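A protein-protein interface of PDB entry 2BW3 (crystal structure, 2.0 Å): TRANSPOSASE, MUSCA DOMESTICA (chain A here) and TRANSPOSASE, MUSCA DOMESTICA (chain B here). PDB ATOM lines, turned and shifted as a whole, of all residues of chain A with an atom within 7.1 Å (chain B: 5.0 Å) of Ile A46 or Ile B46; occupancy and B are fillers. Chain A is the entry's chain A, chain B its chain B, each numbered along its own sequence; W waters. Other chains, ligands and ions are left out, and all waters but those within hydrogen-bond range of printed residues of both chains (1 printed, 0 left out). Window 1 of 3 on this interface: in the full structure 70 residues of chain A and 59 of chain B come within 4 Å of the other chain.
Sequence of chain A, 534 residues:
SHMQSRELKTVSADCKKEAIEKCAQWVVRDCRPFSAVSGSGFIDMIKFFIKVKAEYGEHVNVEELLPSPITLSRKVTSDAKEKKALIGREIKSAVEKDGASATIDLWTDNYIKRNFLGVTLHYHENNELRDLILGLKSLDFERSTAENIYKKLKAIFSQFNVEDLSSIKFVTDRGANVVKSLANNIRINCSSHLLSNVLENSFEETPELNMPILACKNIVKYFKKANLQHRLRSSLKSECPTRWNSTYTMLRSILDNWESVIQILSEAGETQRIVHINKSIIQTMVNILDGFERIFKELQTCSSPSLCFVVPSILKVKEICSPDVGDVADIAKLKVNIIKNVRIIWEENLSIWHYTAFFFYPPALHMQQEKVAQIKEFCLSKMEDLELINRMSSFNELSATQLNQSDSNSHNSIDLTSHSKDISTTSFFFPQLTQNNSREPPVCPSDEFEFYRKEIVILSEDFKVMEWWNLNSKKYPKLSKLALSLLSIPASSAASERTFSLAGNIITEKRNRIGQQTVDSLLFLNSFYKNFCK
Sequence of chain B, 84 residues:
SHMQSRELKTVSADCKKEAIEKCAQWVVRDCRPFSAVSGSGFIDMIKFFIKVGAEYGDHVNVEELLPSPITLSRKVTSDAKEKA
The side-chain amide nitrogen (NE2) of Gln A25 sits at hydrogen-bond distance from the backbone carbonyl oxygen (O) of Lys A22 (2.7 Å).
Among the printed residues, merely in contact across the chains: Lys A22 with Phe B48, Gln A25 with Asp B44, Gln A25 with Met B45, Phe A42 with Met B45, Met A45 with Phe B42, Ile A46 with Ile B46, Ile A46 with Phe B49, Lys A47 with Val B62, Phe A49 with Ile B46, Phe A49 with Ile B50, Ile A50 with Phe B49, Ile A50 with Val B62, Val A62 with Lys B47, Val A62 with Ile B50, Leu A66 with Phe B42 and Leu A66 with Ile B43.
Of the printed residues of chain B, Lys A22 touches Phe B48 (3.7 Å). Ile A46 touches just these residues of chain B: Ile B46 (3.7 Å) and Phe B49 (3.7 Å). Of the printed residues of chain B, Phe A49 touches Ile B46 and Ile B50. Of the printed residues of chain A, Ile B46 touches Ile A46 (3.7 Å) and Phe A49 (3.8 Å). The nearest residue of chain A that does not touch Ile B46 is Val A62 (4.2 Å). The nearest printed residue of chain B that does not touch Gln A25 is Phe B42 (4.9 Å).
Of the 10 printed residues of chain B, 10 touch a printed residue of chain A. Printed residues of chain B that touch a printed residue of chain A: Phe B42, Ile B43, Asp B44, Met B45, Ile B46, Lys B47, Phe B48, Phe B49, Ile B50 and Val B62. Hydrophobic or aromatic side chains of chain B that line the printed part of chain A: Phe B42, Ile B43, Met B45, Ile B46, Phe B48, Phe B49, Ile B50 and Val B62. Hydrophobic or aromatic side chains of chain A that line the printed part of chain B: Phe A42, Met A45, Ile A46, Phe A49, Ile A50, Val A62 and Leu A66. Among the printed residues, 16 pairs touch across the chains.
Water W1 lies within hydrogen-bond range of O of Asp B44 and NZ of Lys A22.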
ATOM      1  N   LYS A  22      -5.528 -24.791  11.245  1.00  0.00           N
ATOM      2  CA  LYS A  22      -4.210 -24.214  11.478  1.00  0.00           C
ATOM      3  C   LYS A  22      -4.194 -23.390  12.754  1.00  0.00           C
ATOM      4  O   LYS A  22      -3.197 -23.406  13.472  1.00  0.00           O
ATOM      5  CB  LYS A  22      -3.729 -23.379  10.280  1.00  0.00           C
ATOM      6  CG  LYS A  22      -3.448 -24.199   9.015  1.00  0.00           C
ATOM      7  CD  LYS A  22      -2.252 -25.151   9.182  1.00  0.00           C
ATOM      8  CE  LYS A  22      -2.018 -25.932   7.879  1.00  0.00           C
ATOM      9  NZ  LYS A  22      -0.816 -26.800   7.954  1.00  0.00           N
ATOM     10  N   GLN A  25      -4.152 -25.875  15.756  1.00  0.00           N
ATOM     11  CA  GLN A  25      -2.841 -26.454  15.998  1.00  0.00           C
ATOM     12  C   GLN A  25      -1.871 -25.390  16.552  1.00  0.00           C
ATOM     13  O   GLN A  25      -0.958 -25.724  17.307  1.00  0.00           O
ATOM     14  CB  GLN A  25      -2.288 -27.171  14.751  1.00  0.00           C
ATOM     15  CG  GLN A  25      -2.079 -26.300  13.504  1.00  0.00           C
ATOM     16  CD  GLN A  25      -0.697 -25.682  13.431  1.00  0.00           C
ATOM     17  OE1 GLN A  25       0.320 -26.403  13.533  1.00  0.00           O
ATOM     18  NE2 GLN A  25      -0.641 -24.337  13.213  1.00  0.00           N
ATOM     19  N   VAL A  37      -6.586 -15.368  18.776  1.00  0.00           N
ATOM     20  CA  VAL A  37      -6.991 -15.346  17.377  1.00  0.00           C
ATOM     21  C   VAL A  37      -7.866 -14.131  17.021  1.00  0.00           C
ATOM     22  O   VAL A  37      -8.042 -13.809  15.856  1.00  0.00           O
ATOM     23  CB  VAL A  37      -7.688 -16.716  17.024  1.00  0.00           C
ATOM     24  CG1 VAL A  37      -9.119 -16.743  17.555  1.00  0.00           C
ATOM     25  CG2 VAL A  37      -7.624 -17.003  15.566  1.00  0.00           C
ATOM     26  N   SER A  40      -6.636  -7.468  17.544  1.00  0.00           N
ATOM     27  CA  SER A  40      -6.564  -6.617  16.363  1.00  0.00           C
ATOM     28  C   SER A  40      -5.130  -6.581  15.809  1.00  0.00           C
ATOM     29  O   SER A  40      -4.925  -6.441  14.601  1.00  0.00           O
ATOM     30  CB  SER A  40      -7.128  -5.217  16.662  1.00  0.00           C
ATOM     31  OG  SER A  40      -6.707  -4.784  17.938  1.00  0.00           O
ATOM     32  N   GLY A  41      -4.132  -6.725  16.676  1.00  0.00           N
ATOM     33  CA  GLY A  41      -2.746  -6.746  16.200  1.00  0.00           C
ATOM     34  C   GLY A  41      -2.528  -8.024  15.386  1.00  0.00           C
ATOM     35  O   GLY A  41      -1.877  -8.019  14.333  1.00  0.00           O
ATOM     36  N   PHE A  42      -3.085  -9.119  15.889  1.00  0.00           N
ATOM     37  CA  PHE A  42      -3.011 -10.424  15.241  1.00  0.00           C
ATOM     38  C   PHE A  42      -3.650 -10.349  13.848  1.00  0.00           C
ATOM     39  O   PHE A  42      -3.052 -10.752  12.853  1.00  0.00           O
ATOM     40  CB  PHE A  42      -3.772 -11.479  16.059  1.00  0.00           C
ATOM     41  CG  PHE A  42      -3.788 -12.841  15.401  1.00  0.00           C
ATOM     42  CD1 PHE A  42      -2.637 -13.633  15.403  1.00  0.00           C
ATOM     43  CD2 PHE A  42      -4.942 -13.318  14.788  1.00  0.00           C
ATOM     44  CE1 PHE A  42      -2.630 -14.895  14.801  1.00  0.00           C
ATOM     45  CE2 PHE A  42      -4.962 -14.594  14.173  1.00  0.00           C
ATOM     46  CZ  PHE A  42      -3.806 -15.382  14.181  1.00  0.00           C
ATOM     47  N   ILE A  43      -4.847  -9.784  13.774  1.00  0.00           N
ATOM     48  CA  ILE A  43      -5.556  -9.657  12.490  1.00  0.00           C
ATOM     49  C   ILE A  43      -4.757  -8.832  11.469  1.00  0.00           C
ATOM     50  O   ILE A  43      -4.660  -9.220  10.298  1.00  0.00           O
ATOM     51  CB  ILE A  43      -6.993  -9.065  12.692  1.00  0.00           C
ATOM     52  CG1 ILE A  43      -7.877 -10.105  13.379  1.00  0.00           C
ATOM     53  CG2 ILE A  43      -7.612  -8.685  11.357  1.00  0.00           C
ATOM     54  CD1 ILE A  43      -9.207  -9.545  13.887  1.00  0.00           C
ATOM     55  N   ASP A  44      -4.158  -7.720  11.897  1.00  0.00           N
ATOM     56  CA  ASP A  44      -3.364  -6.911  10.971  1.00  0.00           C
ATOM     57  C   ASP A  44      -2.089  -7.635  10.519  1.00  0.00           C
ATOM     58  O   ASP A  44      -1.628  -7.464   9.377  1.00  0.00           O
ATOM     59  CB  ASP A  44      -3.034  -5.554  11.584  1.00  0.00           C
ATOM     60  CG  ASP A  44      -4.251  -4.608  11.602  1.00  0.00           C
ATOM     61  OD1 ASP A  44      -5.324  -5.010  11.108  1.00  0.00           O
ATOM     62  OD2 ASP A  44      -4.143  -3.470  12.120  1.00  0.00           O
ATOM     63  N   MET A  45      -1.504  -8.428  11.415  1.00  0.00           N
ATOM     64  CA  MET A  45      -0.312  -9.183  11.068  1.00  0.00           C
ATOM     65  C   MET A  45      -0.690 -10.274  10.027  1.00  0.00           C
ATOM     66  O   MET A  45       0.081 -10.531   9.096  1.00  0.00           O
ATOM     67  CB  MET A  45       0.275  -9.854  12.314  1.00  0.00           C
ATOM     68  CG  MET A  45       1.498 -10.694  11.999  1.00  0.00           C
ATOM     69  SD  MET A  45       2.193 -11.566  13.593  1.00  0.00           S
ATOM     70  CE  MET A  45       3.362 -12.825  12.805  1.00  0.00           C
ATOM     71  N   ILE A  46      -1.819 -10.952  10.228  1.00  0.00           N
ATOM     72  CA  ILE A  46      -2.255 -11.992   9.267  1.00  0.00           C
ATOM     73  C   ILE A  46      -2.516 -11.355   7.892  1.00  0.00           C
ATOM     74  O   ILE A  46      -2.132 -11.914   6.846  1.00  0.00           O
ATOM     75  CB  ILE A  46      -3.472 -12.804   9.773  1.00  0.00           C
ATOM     76  CG1 ILE A  46      -3.078 -13.630  11.014  1.00  0.00           C
ATOM     77  CG2 ILE A  46      -4.061 -13.705   8.632  1.00  0.00           C
ATOM     78  CD1 ILE A  46      -1.752 -14.461  10.834  1.00  0.00           C
ATOM     79  N   LYS A  47      -3.108 -10.167   7.884  1.00  0.00           N
ATOM     80  CA  LYS A  47      -3.324  -9.460   6.621  1.00  0.00           C
ATOM     81  C   LYS A  47      -1.995  -9.225   5.880  1.00  0.00           C
ATOM     82  O   LYS A  47      -1.892  -9.373   4.649  1.00  0.00           O
ATOM     83  CB  LYS A  47      -4.024  -8.145   6.864  1.00  0.00           C
ATOM     84  CG  LYS A  47      -5.481  -8.313   7.275  1.00  0.00           C
ATOM     85  CD  LYS A  47      -6.150  -6.958   7.404  1.00  0.00           C
ATOM     86  CE  LYS A  47      -7.607  -7.104   7.840  1.00  0.00           C
ATOM     87  NZ  LYS A  47      -8.254  -5.773   8.019  1.00  0.00           N
ATOM     88  N   PHE A  48      -0.970  -8.865   6.641  1.00  0.00           N
ATOM     89  CA  PHE A  48       0.347  -8.648   6.081  1.00  0.00           C
ATOM     90  C   PHE A  48       0.923  -9.946   5.470  1.00  0.00           C
ATOM     91  O   PHE A  48       1.426  -9.934   4.350  1.00  0.00           O
ATOM     92  CB  PHE A  48       1.294  -8.111   7.160  1.00  0.00           C
ATOM     93  CG  PHE A  48       2.727  -8.164   6.761  1.00  0.00           C
ATOM     94  CD1 PHE A  48       3.240  -7.247   5.854  1.00  0.00           C
ATOM     95  CD2 PHE A  48       3.551  -9.200   7.230  1.00  0.00           C
ATOM     96  CE1 PHE A  48       4.573  -7.361   5.398  1.00  0.00           C
ATOM     97  CE2 PHE A  48       4.872  -9.322   6.784  1.00  0.00           C
ATOM     98  CZ  PHE A  48       5.382  -8.405   5.866  1.00  0.00           C
ATOM     99  N   PHE A  49       0.867 -11.069   6.184  1.00  0.00           N
ATOM    100  CA  PHE A  49       1.402 -12.297   5.607  1.00  0.00           C
ATOM    101  C   PHE A  49       0.668 -12.775   4.343  1.00  0.00           C
ATOM    102  O   PHE A  49       1.281 -13.353   3.436  1.00  0.00           O
ATOM    103  CB  PHE A  49       1.539 -13.394   6.664  1.00  0.00           C
ATOM    104  CG  PHE A  49       2.656 -13.125   7.630  1.00  0.00           C
ATOM    105  CD1 PHE A  49       2.405 -12.929   8.973  1.00  0.00           C
ATOM    106  CD2 PHE A  49       3.964 -13.017   7.176  1.00  0.00           C
ATOM    107  CE1 PHE A  49       3.456 -12.627   9.847  1.00  0.00           C
ATOM    108  CE2 PHE A  49       5.016 -12.715   8.045  1.00  0.00           C
ATOM    109  CZ  PHE A  49       4.768 -12.522   9.375  1.00  0.00           C
ATOM    110  N   ILE A  50      -0.635 -12.499   4.273  1.00  0.00           N
ATOM    111  CA  ILE A  50      -1.422 -12.858   3.099  1.00  0.00           C
ATOM    112  C   ILE A  50      -0.883 -11.974   1.963  1.00  0.00           C
ATOM    113  O   ILE A  50      -0.649 -12.439   0.846  1.00  0.00           O
ATOM    114  CB  ILE A  50      -2.941 -12.586   3.357  1.00  0.00           C
ATOM    115  CG1 ILE A  50      -3.515 -13.680   4.262  1.00  0.00           C
ATOM    116  CG2 ILE A  50      -3.747 -12.485   2.038  1.00  0.00           C
ATOM    117  CD1 ILE A  50      -4.982 -13.420   4.649  1.00  0.00           C
ATOM    118  N   LYS A  51      -0.599 -10.714   2.285  1.00  0.00           N
ATOM    119  CA  LYS A  51      -0.070  -9.764   1.294  1.00  0.00           C
ATOM    120  C   LYS A  51       1.299 -10.247   0.774  1.00  0.00           C
ATOM    121  O   LYS A  51       1.587 -10.186  -0.433  1.00  0.00           O
ATOM    122  CB  LYS A  51       0.024  -8.345   1.909  1.00  0.00           C
ATOM    123  CG  LYS A  51       0.777  -7.359   1.044  1.00  0.00           C
ATOM    124  CD  LYS A  51       0.663  -5.933   1.604  1.00  0.00           C
ATOM    125  CE  LYS A  51       1.826  -5.059   1.133  1.00  0.00           C
ATOM    126  NZ  LYS A  51       3.134  -5.495   1.733  1.00  0.00           N
ATOM    127  N   VAL A  52       2.115 -10.790   1.667  1.00  0.00           N
ATOM    128  CA  VAL A  52       3.426 -11.323   1.288  1.00  0.00           C
ATOM    129  C   VAL A  52       3.230 -12.506   0.298  1.00  0.00           C
ATOM    130  O   VAL A  52       3.919 -12.610  -0.731  1.00  0.00           O
ATOM    131  CB  VAL A  52       4.224 -11.806   2.554  1.00  0.00           C
ATOM    132  CG1 VAL A  52       5.427 -12.636   2.133  1.00  0.00           C
ATOM    133  CG2 VAL A  52       4.718 -10.596   3.348  1.00  0.00           C
ATOM    134  N   VAL A  62       9.965 -18.791   5.091  1.00  0.00           N
ATOM    135  CA  VAL A  62       9.297 -18.212   6.259  1.00  0.00           C
ATOM    136  C   VAL A  62      10.168 -18.042   7.501  1.00  0.00           C
ATOM    137  O   VAL A  62      10.036 -17.047   8.232  1.00  0.00           O
ATOM    138  CB  VAL A  62       8.032 -19.013   6.601  1.00  0.00           C
ATOM    139  CG1 VAL A  62       7.379 -18.502   7.877  1.00  0.00           C
ATOM    140  CG2 VAL A  62       7.063 -18.947   5.434  1.00  0.00           C
ATOM    141  N   LEU A  65      12.030 -14.848   6.800  1.00  0.00           N
ATOM    142  CA  LEU A  65      11.125 -13.694   6.783  1.00  0.00           C
ATOM    143  C   LEU A  65      10.737 -13.260   8.214  1.00  0.00           C
ATOM    144  O   LEU A  65      10.659 -12.088   8.506  1.00  0.00           O
ATOM    145  CB  LEU A  65       9.848 -14.059   6.003  1.00  0.00           C
ATOM    146  CG  LEU A  65       8.567 -13.223   6.184  1.00  0.00           C
ATOM    147  CD1 LEU A  65       8.774 -11.822   5.643  1.00  0.00           C
ATOM    148  CD2 LEU A  65       7.401 -13.903   5.482  1.00  0.00           C
ATOM    149  N   LEU A  66      10.421 -14.218   9.067  1.00  0.00           N
ATOM    150  CA  LEU A  66      10.012 -13.911  10.427  1.00  0.00           C
ATOM    151  C   LEU A  66      11.089 -13.327  11.294  1.00  0.00           C
ATOM    152  O   LEU A  66      12.238 -13.802  11.294  1.00  0.00           O
ATOM    153  CB  LEU A  66       9.524 -15.165  11.140  1.00  0.00           C
ATOM    154  CG  LEU A  66       8.184 -15.794  10.791  1.00  0.00           C
ATOM    155  CD1 LEU A  66       7.919 -16.897  11.814  1.00  0.00           C
ATOM    156  CD2 LEU A  66       7.082 -14.751  10.857  1.00  0.00           C
ATOM    157  N   PHE B  42       2.912 -21.753  15.384  1.00  0.00           N
ATOM    158  CA  PHE B  42       2.795 -20.420  14.822  1.00  0.00           C
ATOM    159  C   PHE B  42       3.338 -20.371  13.396  1.00  0.00           C
ATOM    160  O   PHE B  42       2.675 -19.870  12.479  1.00  0.00           O
ATOM    161  CB  PHE B  42       3.558 -19.404  15.666  1.00  0.00           C
ATOM    162  CG  PHE B  42       3.551 -18.021  15.077  1.00  0.00           C
ATOM    163  CD1 PHE B  42       2.402 -17.239  15.166  1.00  0.00           C
ATOM    164  CD2 PHE B  42       4.690 -17.498  14.472  1.00  0.00           C
ATOM    165  CE1 PHE B  42       2.388 -15.947  14.668  1.00  0.00           C
ATOM    166  CE2 PHE B  42       4.686 -16.185  13.961  1.00  0.00           C
ATOM    167  CZ  PHE B  42       3.522 -15.425  14.072  1.00  0.00           C
ATOM    168  N   ILE B  43       4.549 -20.895  13.218  1.00  0.00           N
ATOM    169  CA  ILE B  43       5.204 -20.910  11.921  1.00  0.00           C
ATOM    170  C   ILE B  43       4.389 -21.678  10.864  1.00  0.00           C
ATOM    171  O   ILE B  43       4.245 -21.222   9.720  1.00  0.00           O
ATOM    172  CB  ILE B  43       6.640 -21.457  12.067  1.00  0.00           C
ATOM    173  CG1 ILE B  43       7.448 -20.465  12.915  1.00  0.00           C
ATOM    174  CG2 ILE B  43       7.300 -21.605  10.695  1.00  0.00           C
ATOM    175  CD1 ILE B  43       8.782 -21.035  13.481  1.00  0.00           C
ATOM    176  N   ASP B  44       3.873 -22.846  11.232  1.00  0.00           N
ATOM    177  CA  ASP B  44       3.037 -23.599  10.307  1.00  0.00           C
ATOM    178  C   ASP B  44       1.789 -22.818   9.931  1.00  0.00           C
ATOM    179  O   ASP B  44       1.359 -22.853   8.783  1.00  0.00           O
ATOM    180  CB  ASP B  44       2.665 -24.967  10.890  1.00  0.00           C
ATOM    181  CG  ASP B  44       3.782 -25.997  10.704  1.00  0.00           C
ATOM    182  OD1 ASP B  44       4.581 -25.863   9.749  1.00  0.00           O
ATOM    183  OD2 ASP B  44       3.871 -26.941  11.510  1.00  0.00           O
ATOM    184  N   MET B  45       1.234 -22.055  10.872  1.00  0.00           N
ATOM    185  CA  MET B  45       0.041 -21.261  10.588  1.00  0.00           C
ATOM    186  C   MET B  45       0.384 -20.128   9.612  1.00  0.00           C
ATOM    187  O   MET B  45      -0.349 -19.862   8.639  1.00  0.00           O
ATOM    188  CB  MET B  45      -0.572 -20.718  11.881  1.00  0.00           C
ATOM    189  CG  MET B  45      -1.772 -19.805  11.669  1.00  0.00           C
ATOM    190  SD  MET B  45      -2.505 -19.034  13.306  1.00  0.00           S
ATOM    191  CE  MET B  45      -0.904 -18.072  13.898  1.00  0.00           C
ATOM    192  N   ILE B  46       1.497 -19.455   9.865  1.00  0.00           N
ATOM    193  CA  ILE B  46       1.938 -18.374   8.985  1.00  0.00           C
ATOM    194  C   ILE B  46       2.206 -18.921   7.569  1.00  0.00           C
ATOM    195  O   ILE B  46       1.898 -18.246   6.580  1.00  0.00           O
ATOM    196  CB  ILE B  46       3.207 -17.678   9.535  1.00  0.00           C
ATOM    197  CG1 ILE B  46       2.883 -16.983  10.854  1.00  0.00           C
ATOM    198  CG2 ILE B  46       3.736 -16.626   8.542  1.00  0.00           C
ATOM    199  CD1 ILE B  46       1.581 -16.164  10.842  1.00  0.00           C
ATOM    200  N   LYS B  47       2.751 -20.142   7.457  1.00  0.00           N
ATOM    201  CA  LYS B  47       3.005 -20.703   6.124  1.00  0.00           C
ATOM    202  C   LYS B  47       1.696 -20.877   5.383  1.00  0.00           C
ATOM    203  O   LYS B  47       1.635 -20.676   4.159  1.00  0.00           O
ATOM    204  CB  LYS B  47       3.769 -22.032   6.168  1.00  0.00           C
ATOM    205  CG  LYS B  47       5.200 -21.888   6.653  1.00  0.00           C
ATOM    206  CD  LYS B  47       5.897 -23.245   6.792  1.00  0.00           C
ATOM    207  CE  LYS B  47       7.396 -23.044   7.100  1.00  0.00           C
ATOM    208  NZ  LYS B  47       8.089 -24.328   7.364  1.00  0.00           N
ATOM    209  N   PHE B  48       0.652 -21.243   6.121  1.00  0.00           N
ATOM    210  CA  PHE B  48      -0.674 -21.416   5.541  1.00  0.00           C
ATOM    211  C   PHE B  48      -1.212 -20.085   5.025  1.00  0.00           C
ATOM    212  O   PHE B  48      -1.729 -20.006   3.899  1.00  0.00           O
ATOM    213  CB  PHE B  48      -1.643 -22.006   6.566  1.00  0.00           C
ATOM    214  CG  PHE B  48      -3.084 -21.883   6.177  1.00  0.00           C
ATOM    215  CD1 PHE B  48      -3.641 -22.748   5.221  1.00  0.00           C
ATOM    216  CD2 PHE B  48      -3.891 -20.893   6.741  1.00  0.00           C
ATOM    217  CE1 PHE B  48      -4.978 -22.623   4.833  1.00  0.00           C
ATOM    218  CE2 PHE B  48      -5.221 -20.760   6.364  1.00  0.00           C
ATOM    219  CZ  PHE B  48      -5.777 -21.634   5.397  1.00  0.00           C
ATOM    220  N   PHE B  49      -1.079 -19.029   5.823  1.00  0.00           N
ATOM    221  CA  PHE B  49      -1.608 -17.740   5.411  1.00  0.00           C
ATOM    222  C   PHE B  49      -0.892 -17.170   4.203  1.00  0.00           C
ATOM    223  O   PHE B  49      -1.499 -16.449   3.412  1.00  0.00           O
ATOM    224  CB  PHE B  49      -1.678 -16.771   6.603  1.00  0.00           C
ATOM    225  CG  PHE B  49      -2.855 -17.044   7.498  1.00  0.00           C
ATOM    226  CD1 PHE B  49      -2.679 -17.437   8.815  1.00  0.00           C
ATOM    227  CD2 PHE B  49      -4.159 -16.976   6.988  1.00  0.00           C
ATOM    228  CE1 PHE B  49      -3.774 -17.769   9.612  1.00  0.00           C
ATOM    229  CE2 PHE B  49      -5.253 -17.306   7.784  1.00  0.00           C
ATOM    230  CZ  PHE B  49      -5.062 -17.704   9.098  1.00  0.00           C
ATOM    231  N   ILE B  50       0.386 -17.492   4.052  1.00  0.00           N
ATOM    232  CA  ILE B  50       1.151 -17.084   2.871  1.00  0.00           C
ATOM    233  C   ILE B  50       0.555 -17.797   1.638  1.00  0.00           C
ATOM    234  O   ILE B  50       0.390 -17.195   0.547  1.00  0.00           O
ATOM    235  CB  ILE B  50       2.638 -17.430   3.034  1.00  0.00           C
ATOM    236  CG1 ILE B  50       3.276 -16.409   3.992  1.00  0.00           C
ATOM    237  CG2 ILE B  50       3.362 -17.454   1.669  1.00  0.00           C
ATOM    238  CD1 ILE B  50       4.702 -16.729   4.412  1.00  0.00           C
ATOM    239  N   VAL B  62     -10.121 -11.272   5.948  1.00  0.00           N
ATOM    240  CA  VAL B  62      -9.514 -11.985   7.077  1.00  0.00           C
ATOM    241  C   VAL B  62     -10.441 -12.193   8.259  1.00  0.00           C
ATOM    242  O   VAL B  62     -10.495 -13.285   8.812  1.00  0.00           O
ATOM    243  CB  VAL B  62      -8.225 -11.303   7.542  1.00  0.00           C
ATOM    244  CG1 VAL B  62      -7.725 -11.937   8.850  1.00  0.00           C
ATOM    245  CG2 VAL B  62      -7.176 -11.475   6.459  1.00  0.00           C
HETATM  246  O   HOH W   1       1.044 -24.817   7.010  1.00  0.00           O
